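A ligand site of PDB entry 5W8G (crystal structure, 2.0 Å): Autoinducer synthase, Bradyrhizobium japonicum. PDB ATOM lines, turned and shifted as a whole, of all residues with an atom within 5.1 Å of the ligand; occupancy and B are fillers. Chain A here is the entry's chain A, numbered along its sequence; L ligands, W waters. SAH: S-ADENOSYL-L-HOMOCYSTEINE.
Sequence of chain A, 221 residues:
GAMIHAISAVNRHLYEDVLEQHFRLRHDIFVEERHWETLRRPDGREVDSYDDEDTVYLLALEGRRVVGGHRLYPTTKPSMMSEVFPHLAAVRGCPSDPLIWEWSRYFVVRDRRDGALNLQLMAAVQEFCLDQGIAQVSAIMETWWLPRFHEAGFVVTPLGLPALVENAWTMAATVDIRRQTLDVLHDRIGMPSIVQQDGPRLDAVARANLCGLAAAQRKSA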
ATOM      1  N   TRP A  36      -7.851  15.061  14.701  1.00  0.00           N
ATOM      2  CA  TRP A  36      -7.392  15.431  13.367  1.00  0.00           C
ATOM      3  C   TRP A  36      -6.065  16.161  13.534  1.00  0.00           C
ATOM      4  O   TRP A  36      -6.003  17.396  13.464  1.00  0.00           O
ATOM      5  CB  TRP A  36      -8.422  16.289  12.607  1.00  0.00           C
ATOM      6  CG  TRP A  36      -9.721  15.574  12.305  1.00  0.00           C
ATOM      7  CD1 TRP A  36     -10.014  14.259  12.549  1.00  0.00           C
ATOM      8  CD2 TRP A  36     -10.872  16.132  11.666  1.00  0.00           C
ATOM      9  NE1 TRP A  36     -11.294  13.972  12.121  1.00  0.00           N
ATOM     10  CE2 TRP A  36     -11.842  15.102  11.585  1.00  0.00           C
ATOM     11  CE3 TRP A  36     -11.192  17.401  11.176  1.00  0.00           C
ATOM     12  CZ2 TRP A  36     -13.103  15.313  11.013  1.00  0.00           C
ATOM     13  CZ3 TRP A  36     -12.443  17.611  10.606  1.00  0.00           C
ATOM     14  CH2 TRP A  36     -13.384  16.566  10.528  1.00  0.00           C
ATOM     15  N   THR A  38      -3.384  16.693  11.847  1.00  0.00           N
ATOM     16  CA  THR A  38      -2.828  17.585  10.813  1.00  0.00           C
ATOM     17  C   THR A  38      -3.264  19.038  11.033  1.00  0.00           C
ATOM     18  O   THR A  38      -2.627  19.961  10.510  1.00  0.00           O
ATOM     19  CB  THR A  38      -3.135  17.147   9.367  1.00  0.00           C
ATOM     20  OG1 THR A  38      -4.469  17.534   9.000  1.00  0.00           O
ATOM     21  CG2 THR A  38      -2.966  15.633   9.191  1.00  0.00           C
ATOM     22  N   LEU A  39      -4.315  19.241  11.818  1.00  0.00           N
ATOM     23  CA  LEU A  39      -4.847  20.581  12.090  1.00  0.00           C
ATOM     24  C   LEU A  39      -4.365  21.195  13.406  1.00  0.00           C
ATOM     25  O   LEU A  39      -4.748  22.327  13.752  1.00  0.00           O
ATOM     26  CB  LEU A  39      -6.385  20.548  12.071  1.00  0.00           C
ATOM     27  CG  LEU A  39      -7.062  20.062  10.785  1.00  0.00           C
ATOM     28  CD1 LEU A  39      -8.572  19.986  10.995  1.00  0.00           C
ATOM     29  CD2 LEU A  39      -6.707  20.985   9.622  1.00  0.00           C
ATOM     30  N   ASP A  48      -7.270  27.194   9.043  1.00  0.00           N
ATOM     31  CA  ASP A  48      -6.606  26.660   7.858  1.00  0.00           C
ATOM     32  C   ASP A  48      -6.614  27.645   6.671  1.00  0.00           C
ATOM     33  O   ASP A  48      -7.017  28.804   6.832  1.00  0.00           O
ATOM     34  CB  ASP A  48      -7.160  25.258   7.472  1.00  0.00           C
ATOM     35  CG  ASP A  48      -8.576  25.305   6.882  1.00  0.00           C
ATOM     36  OD1 ASP A  48      -9.093  26.404   6.604  1.00  0.00           O
ATOM     37  OD2 ASP A  48      -9.157  24.207   6.688  1.00  0.00           O
ATOM     38  N   SER A  49      -6.188  27.176   5.501  1.00  0.00           N
ATOM     39  CA  SER A  49      -6.089  28.011   4.296  1.00  0.00           C
ATOM     40  C   SER A  49      -7.427  28.533   3.799  1.00  0.00           C
ATOM     41  O   SER A  49      -7.460  29.428   2.941  1.00  0.00           O
ATOM     42  CB  SER A  49      -5.400  27.234   3.172  1.00  0.00           C
ATOM     43  OG  SER A  49      -4.092  26.861   3.561  1.00  0.00           O
ATOM     44  N   TYR A  50      -8.519  27.970   4.308  1.00  0.00           N
ATOM     45  CA  TYR A  50      -9.877  28.332   3.868  1.00  0.00           C
ATOM     46  C   TYR A  50     -10.603  29.207   4.893  1.00  0.00           C
ATOM     47  O   TYR A  50     -11.807  29.430   4.801  1.00  0.00           O
ATOM     48  CB  TYR A  50     -10.668  27.062   3.479  1.00  0.00           C
ATOM     49  CG  TYR A  50      -9.782  26.183   2.628  1.00  0.00           C
ATOM     50  CD1 TYR A  50      -9.456  26.533   1.317  1.00  0.00           C
ATOM     51  CD2 TYR A  50      -9.176  25.048   3.180  1.00  0.00           C
ATOM     52  CE1 TYR A  50      -8.598  25.753   0.560  1.00  0.00           C
ATOM     53  CE2 TYR A  50      -8.318  24.255   2.418  1.00  0.00           C
ATOM     54  CZ  TYR A  50      -8.034  24.616   1.114  1.00  0.00           C
ATOM     55  OH  TYR A  50      -7.180  23.845   0.375  1.00  0.00           O
ATOM     56  N   MET A  80     -10.695  23.123  -0.500  1.00  0.00           N
ATOM     57  CA  MET A  80     -10.186  21.901   0.114  1.00  0.00           C
ATOM     58  C   MET A  80     -10.319  20.711  -0.833  1.00  0.00           C
ATOM     59  O   MET A  80      -9.397  19.886  -0.924  1.00  0.00           O
ATOM     60  CB  MET A  80     -10.914  21.609   1.428  1.00  0.00           C
ATOM     61  CG  MET A  80     -10.151  20.657   2.337  1.00  0.00           C
ATOM     62  SD  MET A  80     -11.206  19.954   3.617  1.00  0.00           S
ATOM     63  CE  MET A  80     -11.691  21.436   4.521  1.00  0.00           C
ATOM     64  N   VAL A  84      -6.734  19.573  -1.708  1.00  0.00           N
ATOM     65  CA  VAL A  84      -6.371  18.498  -0.780  1.00  0.00           C
ATOM     66  C   VAL A  84      -6.926  17.149  -1.224  1.00  0.00           C
ATOM     67  O   VAL A  84      -6.212  16.132  -1.185  1.00  0.00           O
ATOM     68  CB  VAL A  84      -6.813  18.821   0.667  1.00  0.00           C
ATOM     69  CG1 VAL A  84      -6.251  17.794   1.643  1.00  0.00           C
ATOM     70  CG2 VAL A  84      -6.356  20.216   1.066  1.00  0.00           C
ATOM     71  N   PHE A  85      -8.178  17.123  -1.674  1.00  0.00           N
ATOM     72  CA  PHE A  85      -8.836  15.848  -1.985  1.00  0.00           C
ATOM     73  C   PHE A  85      -9.370  15.699  -3.426  1.00  0.00           C
ATOM     74  O   PHE A  85     -10.461  15.138  -3.604  1.00  0.00           O
ATOM     75  CB  PHE A  85      -9.991  15.606  -0.997  1.00  0.00           C
ATOM     76  CG  PHE A  85      -9.575  15.605   0.452  1.00  0.00           C
ATOM     77  CD1 PHE A  85      -8.901  14.520   0.996  1.00  0.00           C
ATOM     78  CD2 PHE A  85      -9.887  16.680   1.279  1.00  0.00           C
ATOM     79  CE1 PHE A  85      -8.531  14.506   2.339  1.00  0.00           C
ATOM     80  CE2 PHE A  85      -9.529  16.672   2.628  1.00  0.00           C
ATOM     81  CZ  PHE A  85      -8.849  15.587   3.151  1.00  0.00           C
ATOM     82  N   TRP A 103     -18.697  23.305   2.041  1.00  0.00           N
ATOM     83  CA  TRP A 103     -19.236  23.290   3.396  1.00  0.00           C
ATOM     84  C   TRP A 103     -18.368  22.409   4.286  1.00  0.00           C
ATOM     85  O   TRP A 103     -18.089  21.261   3.934  1.00  0.00           O
ATOM     86  CB  TRP A 103     -20.659  22.731   3.330  1.00  0.00           C
ATOM     87  CG  TRP A 103     -21.498  22.860   4.571  1.00  0.00           C
ATOM     88  CD1 TRP A 103     -21.525  23.913   5.454  1.00  0.00           C
ATOM     89  CD2 TRP A 103     -22.473  21.924   5.032  1.00  0.00           C
ATOM     90  NE1 TRP A 103     -22.448  23.677   6.437  1.00  0.00           N
ATOM     91  CE2 TRP A 103     -23.041  22.469   6.212  1.00  0.00           C
ATOM     92  CE3 TRP A 103     -22.930  20.690   4.569  1.00  0.00           C
ATOM     93  CZ2 TRP A 103     -24.045  21.802   6.937  1.00  0.00           C
ATOM     94  CZ3 TRP A 103     -23.924  20.021   5.296  1.00  0.00           C
ATOM     95  CH2 TRP A 103     -24.457  20.579   6.468  1.00  0.00           C
ATOM     96  N   SER A 104     -17.927  22.946   5.425  1.00  0.00           N
ATOM     97  CA  SER A 104     -17.005  22.218   6.314  1.00  0.00           C
ATOM     98  C   SER A 104     -17.096  22.664   7.775  1.00  0.00           C
ATOM     99  O   SER A 104     -17.805  23.617   8.116  1.00  0.00           O
ATOM    100  CB  SER A 104     -15.560  22.347   5.828  1.00  0.00           C
ATOM    101  OG  SER A 104     -15.107  23.687   5.881  1.00  0.00           O
ATOM    102  N   ARG A 105     -16.385  21.934   8.638  1.00  0.00           N
ATOM    103  CA  ARG A 105     -16.203  22.275  10.055  1.00  0.00           C
ATOM    104  C   ARG A 105     -17.515  22.356  10.846  1.00  0.00           C
ATOM    105  O   ARG A 105     -17.728  23.278  11.644  1.00  0.00           O
ATOM    106  CB  ARG A 105     -15.371  23.555  10.224  1.00  0.00           C
ATOM    107  CG  ARG A 105     -13.945  23.437   9.690  1.00  0.00           C
ATOM    108  CD  ARG A 105     -13.123  22.337  10.377  1.00  0.00           C
ATOM    109  NE  ARG A 105     -11.697  22.635  10.237  1.00  0.00           N
ATOM    110  CZ  ARG A 105     -10.976  22.374   9.153  1.00  0.00           C
ATOM    111  NH1 ARG A 105     -11.507  21.766   8.093  1.00  0.00           N
ATOM    112  NH2 ARG A 105      -9.692  22.728   9.134  1.00  0.00           N
ATOM    113  N   TYR A 106     -18.387  21.375  10.609  1.00  0.00           N
ATOM    114  CA  TYR A 106     -19.658  21.233  11.333  1.00  0.00           C
ATOM    115  C   TYR A 106     -19.368  20.722  12.739  1.00  0.00           C
ATOM    116  O   TYR A 106     -18.742  19.664  12.900  1.00  0.00           O
ATOM    117  CB  TYR A 106     -20.528  20.228  10.589  1.00  0.00           C
ATOM    118  CG  TYR A 106     -21.989  20.137  10.998  1.00  0.00           C
ATOM    119  CD1 TYR A 106     -22.371  19.598  12.225  1.00  0.00           C
ATOM    120  CD2 TYR A 106     -22.995  20.546  10.124  1.00  0.00           C
ATOM    121  CE1 TYR A 106     -23.716  19.496  12.587  1.00  0.00           C
ATOM    122  CE2 TYR A 106     -24.334  20.446  10.463  1.00  0.00           C
ATOM    123  CZ  TYR A 106     -24.683  19.923  11.691  1.00  0.00           C
ATOM    124  OH  TYR A 106     -26.023  19.842  11.999  1.00  0.00           O
ATOM    125  N   ILE A 140     -16.485  17.284   1.627  1.00  0.00           N
ATOM    126  CA  ILE A 140     -15.708  16.060   1.753  1.00  0.00           C
ATOM    127  C   ILE A 140     -16.112  15.559   3.115  1.00  0.00           C
ATOM    128  O   ILE A 140     -15.787  16.179   4.133  1.00  0.00           O
ATOM    129  CB  ILE A 140     -14.185  16.309   1.703  1.00  0.00           C
ATOM    130  CG1 ILE A 140     -13.776  17.033   0.430  1.00  0.00           C
ATOM    131  CG2 ILE A 140     -13.422  14.993   1.812  1.00  0.00           C
ATOM    132  CD1 ILE A 140     -13.642  18.541   0.601  1.00  0.00           C
ATOM    133  N   MET A 141     -16.854  14.461   3.165  1.00  0.00           N
ATOM    134  CA  MET A 141     -17.338  14.024   4.456  1.00  0.00           C
ATOM    135  C   MET A 141     -17.181  12.538   4.715  1.00  0.00           C
ATOM    136  O   MET A 141     -17.142  11.717   3.785  1.00  0.00           O
ATOM    137  CB  MET A 141     -18.790  14.464   4.690  1.00  0.00           C
ATOM    138  CG  MET A 141     -19.840  13.567   4.068  1.00  0.00           C
ATOM    139  SD  MET A 141     -20.245  14.004   2.377  1.00  0.00           S
ATOM    140  CE  MET A 141     -21.711  13.009   2.142  1.00  0.00           C
ATOM    141  N   GLU A 142     -17.059  12.231   5.999  1.00  0.00           N
ATOM    142  CA  GLU A 142     -17.047  10.847   6.436  1.00  0.00           C
ATOM    143  C   GLU A 142     -18.366  10.207   6.039  1.00  0.00           C
ATOM    144  O   GLU A 142     -19.417  10.841   6.086  1.00  0.00           O
ATOM    145  CB  GLU A 142     -16.821  10.766   7.944  1.00  0.00           C
ATOM    146  CG  GLU A 142     -15.424  11.166   8.358  1.00  0.00           C
ATOM    147  CD  GLU A 142     -15.329  11.514   9.830  1.00  0.00           C
ATOM    148  OE1 GLU A 142     -14.561  10.843  10.543  1.00  0.00           O
ATOM    149  OE2 GLU A 142     -16.003  12.480  10.274  1.00  0.00           O
ATOM    150  N   VAL A 165      -9.417   8.104   4.310  1.00  0.00           N
ATOM    151  CA  VAL A 165      -8.630   9.298   4.621  1.00  0.00           C
ATOM    152  C   VAL A 165      -8.263   9.161   6.087  1.00  0.00           C
ATOM    153  O   VAL A 165      -9.146   9.167   6.957  1.00  0.00           O
ATOM    154  CB  VAL A 165      -9.427  10.603   4.363  1.00  0.00           C
ATOM    155  CG1 VAL A 165      -8.686  11.821   4.922  1.00  0.00           C
ATOM    156  CG2 VAL A 165      -9.693  10.780   2.880  1.00  0.00           C
ATOM    157  N   GLU A 166      -6.979   8.985   6.356  1.00  0.00           N
ATOM    158  CA  GLU A 166      -6.475   8.790   7.723  1.00  0.00           C
ATOM    159  C   GLU A 166      -7.361   7.853   8.543  1.00  0.00           C
ATOM    160  O   GLU A 166      -7.927   8.264   9.560  1.00  0.00           O
ATOM    161  CB  GLU A 166      -6.317  10.145   8.442  1.00  0.00           C
ATOM    162  CG  GLU A 166      -5.232  11.049   7.876  1.00  0.00           C
ATOM    163  CD  GLU A 166      -3.816  10.533   8.130  1.00  0.00           C
ATOM    164  OE1 GLU A 166      -3.593   9.871   9.163  1.00  0.00           O
ATOM    165  OE2 GLU A 166      -2.939  10.803   7.289  1.00  0.00           O
ATOM    166  N   THR A 170     -14.336   8.140   3.635  1.00  0.00           N
ATOM    167  CA  THR A 170     -14.631   9.531   3.320  1.00  0.00           C
ATOM    168  C   THR A 170     -15.044   9.622   1.853  1.00  0.00           C
ATOM    169  O   THR A 170     -14.606   8.808   1.025  1.00  0.00           O
ATOM    170  CB  THR A 170     -13.375  10.398   3.598  1.00  0.00           C
ATOM    171  OG1 THR A 170     -12.887  10.122   4.920  1.00  0.00           O
ATOM    172  CG2 THR A 170     -13.680  11.880   3.498  1.00  0.00           C
HETATM  173  N   SAH L   1     -15.425  17.331   6.400  1.00  0.00           N
HETATM  174  CA  SAH L   1     -14.140  17.706   6.990  1.00  0.00           C
HETATM  175  CB  SAH L   1     -12.997  17.623   5.980  1.00  0.00           C
HETATM  176  CG  SAH L   1     -12.728  16.257   5.332  1.00  0.00           C
HETATM  177  SD  SAH L   1     -12.858  14.866   6.403  1.00  0.00           S
HETATM  178  C   SAH L   1     -14.239  19.119   7.488  1.00  0.00           C
HETATM  179  O   SAH L   1     -15.327  19.607   7.773  1.00  0.00           O
HETATM  180  OXT SAH L   1     -13.243  19.819   7.636  1.00  0.00           O
HETATM  181  C5' SAH L   1     -11.707  15.138   7.718  1.00  0.00           C
HETATM  182  C4' SAH L   1     -10.243  14.937   7.321  1.00  0.00           C
HETATM  183  O4' SAH L   1      -9.827  16.057   6.532  1.00  0.00           O
HETATM  184  C3' SAH L   1      -9.342  14.912   8.545  1.00  0.00           C
HETATM  185  O3' SAH L   1      -8.329  13.902   8.370  1.00  0.00           O
HETATM  186  C2' SAH L   1      -8.685  16.284   8.586  1.00  0.00           C
HETATM  187  O2' SAH L   1      -7.377  16.250   9.156  1.00  0.00           O
HETATM  188  C1' SAH L   1      -8.646  16.633   7.107  1.00  0.00           C
HETATM  189  N9  SAH L   1      -8.650  18.090   6.852  1.00  0.00           N
HETATM  190  C8  SAH L   1      -9.593  18.991   7.195  1.00  0.00           C
HETATM  191  N7  SAH L   1      -9.257  20.234   6.770  1.00  0.00           N
HETATM  192  C5  SAH L   1      -8.071  20.130   6.129  1.00  0.00           C
HETATM  193  C6  SAH L   1      -7.147  21.044   5.430  1.00  0.00           C
HETATM  194  N6  SAH L   1      -7.415  22.357   5.337  1.00  0.00           N
HETATM  195  N1  SAH L   1      -6.016  20.523   4.899  1.00  0.00           N
HETATM  196  C2  SAH L   1      -5.716  19.204   4.991  1.00  0.00           C
HETATM  197  N3  SAH L   1      -6.521  18.318   5.603  1.00  0.00           N
HETATM  198  C4  SAH L   1      -7.684  18.708   6.175  1.00  0.00           C
HETATM  199  O   HOH W   1      -5.418  14.297  10.401  1.00  0.00           O
HETATM  200  O   HOH W   2     -12.174  11.647   7.087  1.00  0.00           O
HETATM  201  O   HOH W   3      -5.786  14.205   7.420  1.00  0.00           O
HETATM  202  O   HOH W   4      -9.742  11.428   8.546  1.00  0.00           O
HETATM  203  O   HOH W   5      -5.157  15.823   5.090  1.00  0.00           O
HETATM  204  O   HOH W   6      -5.244  24.362   4.789  1.00  0.00           O
HETATM  205  O   HOH W   7      -3.970  21.646   3.433  1.00  0.00           O
HETATM  206  O   HOH W   8     -16.308  19.279   3.958  1.00  0.00           O
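The backbone carbonyl oxygen of Met 80 sits at hydrogen-bond distance from the backbone NH of Phe 85, at 3.1 Å.
The side-chain carboxylate (OD1) of Asp 48 is in hydrogen-bond range of the backbone NH (N) of Tyr 50 (2.8 Å).
The side-chain carboxylate (OD2) of Asp 48 lies within salt-bridge range of the guanidinium group (NH2) of Arg 105, 2.9 Å away.
SD of Met 80 lies close to N7 of the ligand (3.7 Å).
Residues that only touch the ligand: Ser 104 (3.4 Å), Phe 85 (3.6 Å), Trp 36 (3.6 Å), Tyr 50 (3.6 Å), Val 84 (3.7 Å) and Leu 39 (3.8 Å).
11 residues have an atom within 4 Å of the ligand: Trp 36, Thr 38, Leu 39, Asp 48, Tyr 50, Met 80, Val 84, Phe 85, Ser 104, Arg 105 and Ile 140.
O of Ile 140 lies within hydrogen-bond range of N of the ligand (2.6 Å).
OG1 of Thr 38 sits at hydrogen-bond distance from O2' of the ligand, 3.2 Å away.
The backbone NH (N) of Arg 105 sits at hydrogen-bond distance from an oxygen (O) of the ligand.
The side-chain carboxylate (OD2) of Asp 48 lies within hydrogen-bond range of a nitrogen (N6) of the ligand (2.9 Å).
An oxygen (OXT) of the ligand is in salt-bridge range of the guanidinium group (NH1) of Arg 105 (2.6 Å).
Water W4 lies within hydrogen-bond range of the backbone carbonyl oxygen of Val 165 (2.8 Å) and an oxygen (O3') of the ligand (2.9 Å).
Water W6 bridges N6 of the ligand (3.0 Å) and OG of Ser 49 (3.0 Å).
Water W1 lies within hydrogen-bond range of an oxygen (O2') of the ligand (3.0 Å) and the backbone NH of Thr 38 (3.5 Å).
Water W8 lies within hydrogen-bond range of O of Trp 103 (2.7 Å), N of Ile 140 (3.1 Å) and N of the ligand (3.2 Å).
Water W2 lies within hydrogen-bond range of OG1 of Thr 170 (2.7 Å) and SD of the ligand (3.4 Å).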
